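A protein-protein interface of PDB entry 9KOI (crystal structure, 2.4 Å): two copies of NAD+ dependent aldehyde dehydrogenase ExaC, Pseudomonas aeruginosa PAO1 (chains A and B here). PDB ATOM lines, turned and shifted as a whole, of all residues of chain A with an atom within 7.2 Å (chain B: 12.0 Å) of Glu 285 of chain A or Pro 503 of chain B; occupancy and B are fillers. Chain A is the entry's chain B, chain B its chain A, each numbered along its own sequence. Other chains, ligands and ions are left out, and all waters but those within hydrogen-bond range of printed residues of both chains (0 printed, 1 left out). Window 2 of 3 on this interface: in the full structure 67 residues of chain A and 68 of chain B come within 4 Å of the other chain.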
ATOM      1  N   GLU A 280       1.583  32.015   9.592  1.00  0.00           N
ATOM      2  CA  GLU A 280       1.256  31.865   8.184  1.00  0.00           C
ATOM      3  C   GLU A 280       0.555  30.525   7.943  1.00  0.00           C
ATOM      4  O   GLU A 280       0.785  29.555   8.671  1.00  0.00           O
ATOM      5  CB  GLU A 280       2.511  31.966   7.316  1.00  0.00           C
ATOM      6  CG  GLU A 280       3.705  31.142   7.784  1.00  0.00           C
ATOM      7  CD  GLU A 280       4.457  31.786   8.935  1.00  0.00           C
ATOM      8  OE1 GLU A 280       4.899  32.943   8.785  1.00  0.00           O
ATOM      9  OE2 GLU A 280       4.604  31.132   9.990  1.00  0.00           O
ATOM     10  N   PRO A 281      -0.319  30.453   6.934  1.00  0.00           N
ATOM     11  CA  PRO A 281      -1.011  29.184   6.649  1.00  0.00           C
ATOM     12  C   PRO A 281      -0.071  28.019   6.402  1.00  0.00           C
ATOM     13  O   PRO A 281      -0.436  26.869   6.679  1.00  0.00           O
ATOM     14  CB  PRO A 281      -1.842  29.512   5.400  1.00  0.00           C
ATOM     15  CG  PRO A 281      -2.036  30.989   5.457  1.00  0.00           C
ATOM     16  CD  PRO A 281      -0.779  31.544   6.056  1.00  0.00           C
ATOM     17  N   ALA A 282       1.130  28.279   5.884  1.00  0.00           N
ATOM     18  CA  ALA A 282       2.070  27.193   5.637  1.00  0.00           C
ATOM     19  C   ALA A 282       2.601  26.612   6.941  1.00  0.00           C
ATOM     20  O   ALA A 282       2.825  25.400   7.033  1.00  0.00           O
ATOM     21  CB  ALA A 282       3.212  27.691   4.756  1.00  0.00           C
ATOM     22  N   PHE A 283       2.775  27.451   7.963  1.00  0.00           N
ATOM     23  CA  PHE A 283       3.198  26.963   9.272  1.00  0.00           C
ATOM     24  C   PHE A 283       2.147  26.037   9.871  1.00  0.00           C
ATOM     25  O   PHE A 283       2.471  24.963  10.392  1.00  0.00           O
ATOM     26  CB  PHE A 283       3.470  28.147  10.202  1.00  0.00           C
ATOM     27  CG  PHE A 283       3.994  27.758  11.557  1.00  0.00           C
ATOM     28  CD1 PHE A 283       5.334  27.464  11.739  1.00  0.00           C
ATOM     29  CD2 PHE A 283       3.145  27.695  12.652  1.00  0.00           C
ATOM     30  CE1 PHE A 283       5.818  27.113  12.985  1.00  0.00           C
ATOM     31  CE2 PHE A 283       3.623  27.344  13.899  1.00  0.00           C
ATOM     32  CZ  PHE A 283       4.962  27.052  14.066  1.00  0.00           C
ATOM     33  N   ILE A 284       0.880  26.466   9.835  1.00  0.00           N
ATOM     34  CA  ILE A 284      -0.240  25.639  10.287  1.00  0.00           C
ATOM     35  C   ILE A 284      -0.132  24.224   9.729  1.00  0.00           C
ATOM     36  O   ILE A 284      -0.328  23.237  10.448  1.00  0.00           O
ATOM     37  CB  ILE A 284      -1.577  26.300   9.909  1.00  0.00           C
ATOM     38  CG1 ILE A 284      -1.689  27.672  10.580  1.00  0.00           C
ATOM     39  CG2 ILE A 284      -2.747  25.415  10.311  1.00  0.00           C
ATOM     40  CD1 ILE A 284      -2.897  28.476  10.150  1.00  0.00           C
ATOM     41  N   GLU A 285       0.166  24.102   8.432  1.00  0.00           N
ATOM     42  CA  GLU A 285       0.284  22.777   7.826  1.00  0.00           C
ATOM     43  C   GLU A 285       1.424  21.982   8.447  1.00  0.00           C
ATOM     44  O   GLU A 285       1.268  20.797   8.761  1.00  0.00           O
ATOM     45  CB  GLU A 285       0.509  22.892   6.317  1.00  0.00           C
ATOM     46  CG  GLU A 285      -0.721  22.788   5.446  1.00  0.00           C
ATOM     47  CD  GLU A 285      -0.391  23.003   3.980  1.00  0.00           C
ATOM     48  OE1 GLU A 285       0.504  22.298   3.469  1.00  0.00           O
ATOM     49  OE2 GLU A 285      -1.018  23.875   3.343  1.00  0.00           O
ATOM     50  N   LYS A 286       2.587  22.620   8.629  1.00  0.00           N
ATOM     51  CA  LYS A 286       3.726  21.927   9.226  1.00  0.00           C
ATOM     52  C   LYS A 286       3.393  21.403  10.616  1.00  0.00           C
ATOM     53  O   LYS A 286       3.837  20.315  11.000  1.00  0.00           O
ATOM     54  CB  LYS A 286       4.940  22.855   9.286  1.00  0.00           C
ATOM     55  CG  LYS A 286       6.225  22.138   9.667  1.00  0.00           C
ATOM     56  CD  LYS A 286       7.337  23.104  10.034  1.00  0.00           C
ATOM     57  CE  LYS A 286       8.663  22.371  10.168  1.00  0.00           C
ATOM     58  NZ  LYS A 286       9.689  23.181  10.882  1.00  0.00           N
ATOM     59  N   ALA A 287       2.613  22.165  11.386  1.00  0.00           N
ATOM     60  CA  ALA A 287       2.229  21.716  12.719  1.00  0.00           C
ATOM     61  C   ALA A 287       1.269  20.536  12.640  1.00  0.00           C
ATOM     62  O   ALA A 287       1.469  19.515  13.308  1.00  0.00           O
ATOM     63  CB  ALA A 287       1.605  22.874  13.498  1.00  0.00           C
ATOM     64  N   ALA A 288       0.214  20.661  11.828  1.00  0.00           N
ATOM     65  CA  ALA A 288      -0.698  19.541  11.616  1.00  0.00           C
ATOM     66  C   ALA A 288       0.038  18.330  11.059  1.00  0.00           C
ATOM     67  O   ALA A 288      -0.251  17.189  11.438  1.00  0.00           O
ATOM     68  CB  ALA A 288      -1.834  19.957  10.683  1.00  0.00           C
ATOM     69  N   GLU A 289       0.986  18.558  10.147  1.00  0.00           N
ATOM     70  CA  GLU A 289       1.870  17.484   9.708  1.00  0.00           C
ATOM     71  C   GLU A 289       2.627  16.889  10.887  1.00  0.00           C
ATOM     72  O   GLU A 289       2.715  15.664  11.032  1.00  0.00           O
ATOM     73  CB  GLU A 289       2.849  18.005   8.660  1.00  0.00           C
ATOM     74  CG  GLU A 289       4.057  17.116   8.483  1.00  0.00           C
ATOM     75  CD  GLU A 289       4.955  17.594   7.373  1.00  0.00           C
ATOM     76  OE1 GLU A 289       5.654  18.604   7.580  1.00  0.00           O
ATOM     77  OE2 GLU A 289       4.976  16.954   6.304  1.00  0.00           O
ATOM     78  N   GLY A 290       3.189  17.750  11.740  1.00  0.00           N
ATOM     79  CA  GLY A 290       3.961  17.284  12.877  1.00  0.00           C
ATOM     80  C   GLY A 290       3.182  16.379  13.804  1.00  0.00           C
ATOM     81  O   GLY A 290       3.783  15.578  14.527  1.00  0.00           O
ATOM     82  N   LEU A 291       1.852  16.485  13.800  1.00  0.00           N
ATOM     83  CA  LEU A 291       1.026  15.561  14.568  1.00  0.00           C
ATOM     84  C   LEU A 291       0.829  14.248  13.819  1.00  0.00           C
ATOM     85  O   LEU A 291       0.947  13.172  14.414  1.00  0.00           O
ATOM     86  CB  LEU A 291      -0.324  16.206  14.889  1.00  0.00           C
ATOM     87  CG  LEU A 291      -1.114  15.641  16.075  1.00  0.00           C
ATOM     88  CD1 LEU A 291      -2.058  16.697  16.622  1.00  0.00           C
ATOM     89  CD2 LEU A 291      -1.889  14.382  15.703  1.00  0.00           C
ATOM     90  N   PHE A 318      -7.756  23.563  14.845  1.00  0.00           N
ATOM     91  CA  PHE A 318      -6.509  22.884  14.504  1.00  0.00           C
ATOM     92  C   PHE A 318      -6.753  21.456  14.034  1.00  0.00           C
ATOM     93  O   PHE A 318      -6.213  21.033  13.005  1.00  0.00           O
ATOM     94  CB  PHE A 318      -5.554  22.899  15.696  1.00  0.00           C
ATOM     95  CG  PHE A 318      -4.237  22.243  15.419  1.00  0.00           C
ATOM     96  CD1 PHE A 318      -3.397  22.740  14.437  1.00  0.00           C
ATOM     97  CD2 PHE A 318      -3.844  21.122  16.129  1.00  0.00           C
ATOM     98  CE1 PHE A 318      -2.184  22.135  14.175  1.00  0.00           C
ATOM     99  CE2 PHE A 318      -2.631  20.513  15.871  1.00  0.00           C
ATOM    100  CZ  PHE A 318      -1.801  21.020  14.892  1.00  0.00           C
ATOM    101  N   GLU A 321      -7.440  20.892  10.508  1.00  0.00           N
ATOM    102  CA  GLU A 321      -6.263  20.797   9.653  1.00  0.00           C
ATOM    103  C   GLU A 321      -5.576  19.442   9.795  1.00  0.00           C
ATOM    104  O   GLU A 321      -5.090  18.880   8.806  1.00  0.00           O
ATOM    105  CB  GLU A 321      -5.285  21.925   9.982  1.00  0.00           C
ATOM    106  CG  GLU A 321      -5.830  23.316   9.713  1.00  0.00           C
ATOM    107  CD  GLU A 321      -6.125  23.551   8.246  1.00  0.00           C
ATOM    108  OE1 GLU A 321      -5.453  22.927   7.396  1.00  0.00           O
ATOM    109  OE2 GLU A 321      -7.028  24.357   7.939  1.00  0.00           O
ATOM    110  N   LYS A 324      -7.590  16.629   7.909  1.00  0.00           N
ATOM    111  CA  LYS A 324      -7.439  16.655   6.456  1.00  0.00           C
ATOM    112  C   LYS A 324      -6.241  15.825   6.017  1.00  0.00           C
ATOM    113  O   LYS A 324      -6.306  15.103   5.014  1.00  0.00           O
ATOM    114  CB  LYS A 324      -7.301  18.094   5.957  1.00  0.00           C
ATOM    115  CG  LYS A 324      -6.455  18.213   4.694  1.00  0.00           C
ATOM    116  CD  LYS A 324      -6.871  19.383   3.821  1.00  0.00           C
ATOM    117  CE  LYS A 324      -6.195  19.302   2.459  1.00  0.00           C
ATOM    118  NZ  LYS A 324      -5.704  20.628   1.991  1.00  0.00           N
ATOM    119  N   LYS A 325      -5.142  15.899   6.768  1.00  0.00           N
ATOM    120  CA  LYS A 325      -3.932  15.177   6.397  1.00  0.00           C
ATOM    121  C   LYS A 325      -3.994  13.716   6.818  1.00  0.00           C
ATOM    122  O   LYS A 325      -3.434  12.856   6.128  1.00  0.00           O
ATOM    123  CB  LYS A 325      -2.709  15.875   6.989  1.00  0.00           C
ATOM    124  CG  LYS A 325      -2.325  17.116   6.199  1.00  0.00           C
ATOM    125  CD  LYS A 325      -1.119  17.830   6.768  1.00  0.00           C
ATOM    126  CE  LYS A 325      -0.782  19.040   5.914  1.00  0.00           C
ATOM    127  NZ  LYS A 325       0.110  18.675   4.779  1.00  0.00           N
ATOM    128  N   TRP A 436       5.182  23.467  19.650  1.00  0.00           N
ATOM    129  CA  TRP A 436       4.834  24.306  18.507  1.00  0.00           C
ATOM    130  C   TRP A 436       4.281  25.629  19.018  1.00  0.00           C
ATOM    131  O   TRP A 436       3.143  25.690  19.500  1.00  0.00           O
ATOM    132  CB  TRP A 436       3.829  23.603  17.598  1.00  0.00           C
ATOM    133  CG  TRP A 436       4.373  22.356  16.975  1.00  0.00           C
ATOM    134  CD1 TRP A 436       4.461  21.121  17.552  1.00  0.00           C
ATOM    135  CD2 TRP A 436       4.911  22.220  15.655  1.00  0.00           C
ATOM    136  NE1 TRP A 436       5.018  20.226  16.670  1.00  0.00           N
ATOM    137  CE2 TRP A 436       5.304  20.876  15.498  1.00  0.00           C
ATOM    138  CE3 TRP A 436       5.098  23.106  14.589  1.00  0.00           C
ATOM    139  CZ2 TRP A 436       5.871  20.397  14.320  1.00  0.00           C
ATOM    140  CZ3 TRP A 436       5.663  22.629  13.420  1.00  0.00           C
ATOM    141  CH2 TRP A 436       6.041  21.287  13.295  1.00  0.00           C
ATOM    142  N   SER B 146      18.276  26.060   8.434  1.00  0.00           N
ATOM    143  CA  SER B 146      17.102  26.319   9.258  1.00  0.00           C
ATOM    144  C   SER B 146      16.944  25.289  10.371  1.00  0.00           C
ATOM    145  O   SER B 146      15.842  25.122  10.901  1.00  0.00           O
ATOM    146  CB  SER B 146      15.840  26.381   8.395  1.00  0.00           C
ATOM    147  OG  SER B 146      15.620  25.161   7.713  1.00  0.00           O
ATOM    148  N   THR B 147      18.019  24.587  10.733  1.00  0.00           N
ATOM    149  CA  THR B 147      17.982  23.571  11.780  1.00  0.00           C
ATOM    150  C   THR B 147      19.185  23.778  12.685  1.00  0.00           C
ATOM    151  O   THR B 147      20.331  23.680  12.232  1.00  0.00           O
ATOM    152  CB  THR B 147      17.990  22.157  11.192  1.00  0.00           C
ATOM    153  OG1 THR B 147      17.006  22.060  10.155  1.00  0.00           O
ATOM    154  CG2 THR B 147      17.686  21.129  12.272  1.00  0.00           C
ATOM    155  N   SER B 498      13.749  24.055  14.567  1.00  0.00           N
ATOM    156  CA  SER B 498      13.656  24.360  13.147  1.00  0.00           C
ATOM    157  C   SER B 498      13.083  25.760  12.972  1.00  0.00           C
ATOM    158  O   SER B 498      12.086  26.111  13.611  1.00  0.00           O
ATOM    159  CB  SER B 498      12.780  23.339  12.422  1.00  0.00           C
ATOM    160  OG  SER B 498      12.640  23.669  11.051  1.00  0.00           O
ATOM    161  N   TYR B 499      13.717  26.557  12.115  1.00  0.00           N
ATOM    162  CA  TYR B 499      13.251  27.904  11.819  1.00  0.00           C
ATOM    163  C   TYR B 499      12.575  27.995  10.460  1.00  0.00           C
ATOM    164  O   TYR B 499      12.216  29.094  10.025  1.00  0.00           O
ATOM    165  CB  TYR B 499      14.414  28.890  11.902  1.00  0.00           C
ATOM    166  CG  TYR B 499      15.112  28.836  13.234  1.00  0.00           C
ATOM    167  CD1 TYR B 499      14.594  29.496  14.338  1.00  0.00           C
ATOM    168  CD2 TYR B 499      16.274  28.097  13.397  1.00  0.00           C
ATOM    169  CE1 TYR B 499      15.223  29.436  15.565  1.00  0.00           C
ATOM    170  CE2 TYR B 499      16.909  28.033  14.618  1.00  0.00           C
ATOM    171  CZ  TYR B 499      16.383  28.703  15.698  1.00  0.00           C
ATOM    172  OH  TYR B 499      17.018  28.639  16.916  1.00  0.00           O
ATOM    173  N   ASP B 500      12.393  26.865   9.785  1.00  0.00           N
ATOM    174  CA  ASP B 500      11.661  26.821   8.531  1.00  0.00           C
ATOM    175  C   ASP B 500      10.189  26.571   8.811  1.00  0.00           C
ATOM    176  O   ASP B 500       9.838  25.696   9.608  1.00  0.00           O
ATOM    177  CB  ASP B 500      12.209  25.726   7.615  1.00  0.00           C
ATOM    178  CG  ASP B 500      11.716  25.864   6.184  1.00  0.00           C
ATOM    179  OD1 ASP B 500      10.880  26.751   5.919  1.00  0.00           O
ATOM    180  OD2 ASP B 500      12.153  25.070   5.324  1.00  0.00           O
ATOM    181  N   ILE B 501       9.331  27.343   8.151  1.00  0.00           N
ATOM    182  CA  ILE B 501       7.893  27.164   8.277  1.00  0.00           C
ATOM    183  C   ILE B 501       7.520  26.213   7.149  1.00  0.00           C
ATOM    184  O   ILE B 501       8.410  25.651   6.504  1.00  0.00           O
ATOM    185  CB  ILE B 501       7.143  28.507   8.204  1.00  0.00           C
ATOM    186  CG1 ILE B 501       7.435  29.219   6.883  1.00  0.00           C
ATOM    187  CG2 ILE B 501       7.560  29.400   9.353  1.00  0.00           C
ATOM    188  CD1 ILE B 501       6.274  29.237   5.927  1.00  0.00           C
ATOM    189  N   ASN B 502       6.221  25.998   6.925  1.00  0.00           N
ATOM    190  CA  ASN B 502       5.670  25.141   5.870  1.00  0.00           C
ATOM    191  C   ASN B 502       6.076  23.676   6.056  1.00  0.00           C
ATOM    192  O   ASN B 502       7.065  23.383   6.741  1.00  0.00           O
ATOM    193  CB  ASN B 502       6.038  25.703   4.478  1.00  0.00           C
ATOM    194  CG  ASN B 502       7.427  25.300   3.979  1.00  0.00           C
ATOM    195  OD1 ASN B 502       7.848  24.147   4.068  1.00  0.00           O
ATOM    196  ND2 ASN B 502       8.148  26.278   3.442  1.00  0.00           N
ATOM    197  N   PRO B 503       5.335  22.728   5.486  1.00  0.00           N
ATOM    198  CA  PRO B 503       5.600  21.313   5.763  1.00  0.00           C
ATOM    199  C   PRO B 503       6.707  20.730   4.895  1.00  0.00           C
ATOM    200  O   PRO B 503       7.070  21.258   3.843  1.00  0.00           O
ATOM    201  CB  PRO B 503       4.260  20.629   5.457  1.00  0.00           C
ATOM    202  CG  PRO B 503       3.382  21.687   4.830  1.00  0.00           C
ATOM    203  CD  PRO B 503       4.225  22.876   4.531  1.00  0.00           C
ATOM    204  N   LEU B 504       7.249  19.611   5.378  1.00  0.00           N
ATOM    205  CA  LEU B 504       8.374  18.923   4.763  1.00  0.00           C
ATOM    206  C   LEU B 504       7.949  17.828   3.781  1.00  0.00           C
ATOM    207  O   LEU B 504       8.768  16.970   3.430  1.00  0.00           O
ATOM    208  CB  LEU B 504       9.299  18.373   5.850  1.00  0.00           C
ATOM    209  CG  LEU B 504       8.634  17.774   7.096  1.00  0.00           C
ATOM    210  CD1 LEU B 504       8.017  16.423   6.831  1.00  0.00           C
ATOM    211  CD2 LEU B 504       9.610  17.696   8.260  1.00  0.00           C
ATOM    212  N   GLY B 505       6.691  17.838   3.332  1.00  0.00           N
ATOM    213  CA  GLY B 505       6.226  16.933   2.297  1.00  0.00           C
ATOM    214  C   GLY B 505       5.832  15.538   2.736  1.00  0.00           C
ATOM    215  O   GLY B 505       5.103  14.862   1.999  1.00  0.00           O
ATOM    216  N   PHE B 506       6.286  15.069   3.896  1.00  0.00           N
ATOM    217  CA  PHE B 506       5.754  13.824   4.433  1.00  0.00           C
ATOM    218  C   PHE B 506       4.274  13.993   4.777  1.00  0.00           C
ATOM    219  O   PHE B 506       3.754  15.107   4.847  1.00  0.00           O
ATOM    220  CB  PHE B 506       6.547  13.387   5.668  1.00  0.00           C
ATOM    221  CG  PHE B 506       7.966  12.957   5.372  1.00  0.00           C
ATOM    222  CD1 PHE B 506       8.928  13.884   5.005  1.00  0.00           C
ATOM    223  CD2 PHE B 506       8.341  11.627   5.481  1.00  0.00           C
ATOM    224  CE1 PHE B 506      10.227  13.502   4.746  1.00  0.00           C
ATOM    225  CE2 PHE B 506       9.643  11.235   5.219  1.00  0.00           C
ATOM    226  CZ  PHE B 506      10.587  12.175   4.851  1.00  0.00           C
ATOM    227  N   PHE B 507       3.593  12.860   4.963  1.00  0.00           N
ATOM    228  CA  PHE B 507       2.242  12.782   5.556  1.00  0.00           C
ATOM    229  C   PHE B 507       1.238  13.871   5.161  1.00  0.00           C
ATOM    230  O   PHE B 507       1.295  15.018   5.609  1.00  0.00           O
ATOM    231  CB  PHE B 507       2.351  12.751   7.079  1.00  0.00           C
ATOM    232  CG  PHE B 507       2.863  11.453   7.619  1.00  0.00           C
ATOM    233  CD1 PHE B 507       2.203  10.269   7.337  1.00  0.00           C
ATOM    234  CD2 PHE B 507       3.997  11.410   8.408  1.00  0.00           C
ATOM    235  CE1 PHE B 507       2.665   9.068   7.827  1.00  0.00           C
ATOM    236  CE2 PHE B 507       4.464  10.212   8.903  1.00  0.00           C
ATOM    237  CZ  PHE B 507       3.797   9.040   8.610  1.00  0.00           C
ATOM    238  OXT PHE B 507       0.303  13.610   4.405  1.00  0.00           O
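The chain-end carboxylate (O) of Phe 507 of chain B is in salt-bridge range of the side-chain amino group (NZ) of Lys 325 of chain A (3.9 Å). O of Asp 500 of chain B lies within hydrogen-bond range of NZ of Lys 286 of chain A. OE2 of Glu 289 of chain A lies within hydrogen-bond range of N of Phe 506 of chain B. The side-chain amino group of Lys 286 of chain A is in hydrogen-bond range of the side-chain hydroxyl of Ser 498 of chain B, 3.0 Å away. The backbone NH (N) of Asn 502 of chain B lies close to the backbone carbonyl oxygen (O) of Ala 282 of chain A, 3.4 Å away. The backbone NH (N) of Leu 504 of chain B lies within hydrogen-bond range of the side-chain carboxylate (OE1) of Glu 289 of chain A (2.9 Å).
OG of Ser 498 of chain B sits close to N of Asp 500 of chain B (3.4 Å). NZ of Lys 325 of chain A is in salt-bridge range of OE1 of Glu 285 of chain A.
Glu 280 of chain A touches Ile 501 of chain B (OE2 to CG2, 3.5 Å). Ala 282 of chain A touches Ile 501 of chain B (CB to CD1, 3.6 Å). Ala 282 of chain A touches Pro 503 of chain B. CD1 of Phe 283 of chain A touches CG2 of Ile 501 of chain B (3.8 Å). N of Asn 502 of chain B touches N of Phe 283 of chain A (3.9 Å). Glu 285 of chain A touches Pro 503 of chain B (OE1 to CG, 3.2 Å). O of Asn 502 of chain B touches CG of Lys 286 of chain A (3.3 Å). Pro 503 of chain B touches Lys 286 of chain A. Pro 503 of chain B touches Glu 289 of chain A (CB to OE1, 3.2 Å). N of Gly 505 of chain B touches OE2 of Glu 289 of chain A, at 3.5 Å.
No residue of chain B comes within 4 Å of Pro 281 of chain A. Of chain B, only Ile 501, Asn 502 and Pro 503 come within 4 Å of Ala 282 of chain A. No residue of chain B comes within 4 Å of Ile 284 of chain A. Of the printed residues of chain B, Lys 286 of chain A touches Ser 498, Asp 500, Asn 502 and Pro 503. No residue of chain B comes within 4 Å of Ala 288 of chain A. Of the printed residues of chain B, Glu 289 of chain A touches Pro 503 (3.2 Å), Leu 504 (2.9 Å), Gly 505 (3.5 Å) and Phe 506 (2.7 Å). Phe 318 of chain A touches none of the printed residues of chain B. Of the printed residues of chain A, Ser 498 of chain B touches Lys 286. Of the printed residues of chain A, Ile 501 of chain B touches Glu 280 (3.5 Å), Ala 282 (3.6 Å) and Phe 283 (3.8 Å). Pro 503 of chain B touches just these residues of chain A: Ala 282 (3.8 Å), Glu 285 (3.2 Å), Lys 286 (3.8 Å) and Glu 289 (3.2 Å). Of the printed residues of chain A, Leu 504 of chain B touches Glu 289 (2.9 Å). Of the printed residues of chain A, Phe 506 of chain B touches Glu 289 (2.7 Å).
Of the 12 printed residues of chain B, 9 touch a printed residue of chain A. Printed residues of chain B that touch a printed residue of chain A: Ser 498, Asp 500, Ile 501, Asn 502, Pro 503, Leu 504, Gly 505, Phe 506 and Phe 507. Of the 17 printed residues of chain A, 7 touch a printed residue of chain B. Printed residues of chain A that touch a printed residue of chain B: Glu 280, Ala 282, Phe 283, Glu 285, Lys 286, Glu 289 and Lys 325. Hydrophobic or aromatic side chains of chain A that line the printed part of chain B: Ala 282 and Phe 283. Among the printed residues, no Asp or Glu carboxylate lies within 4 Å of a Lys or Arg side-chain nitrogen of the other chain.
No position is printed for both chains. Of the 16 pairs that touch across the chains among the printed residues, none has its exchanged pair printed and touching as well.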
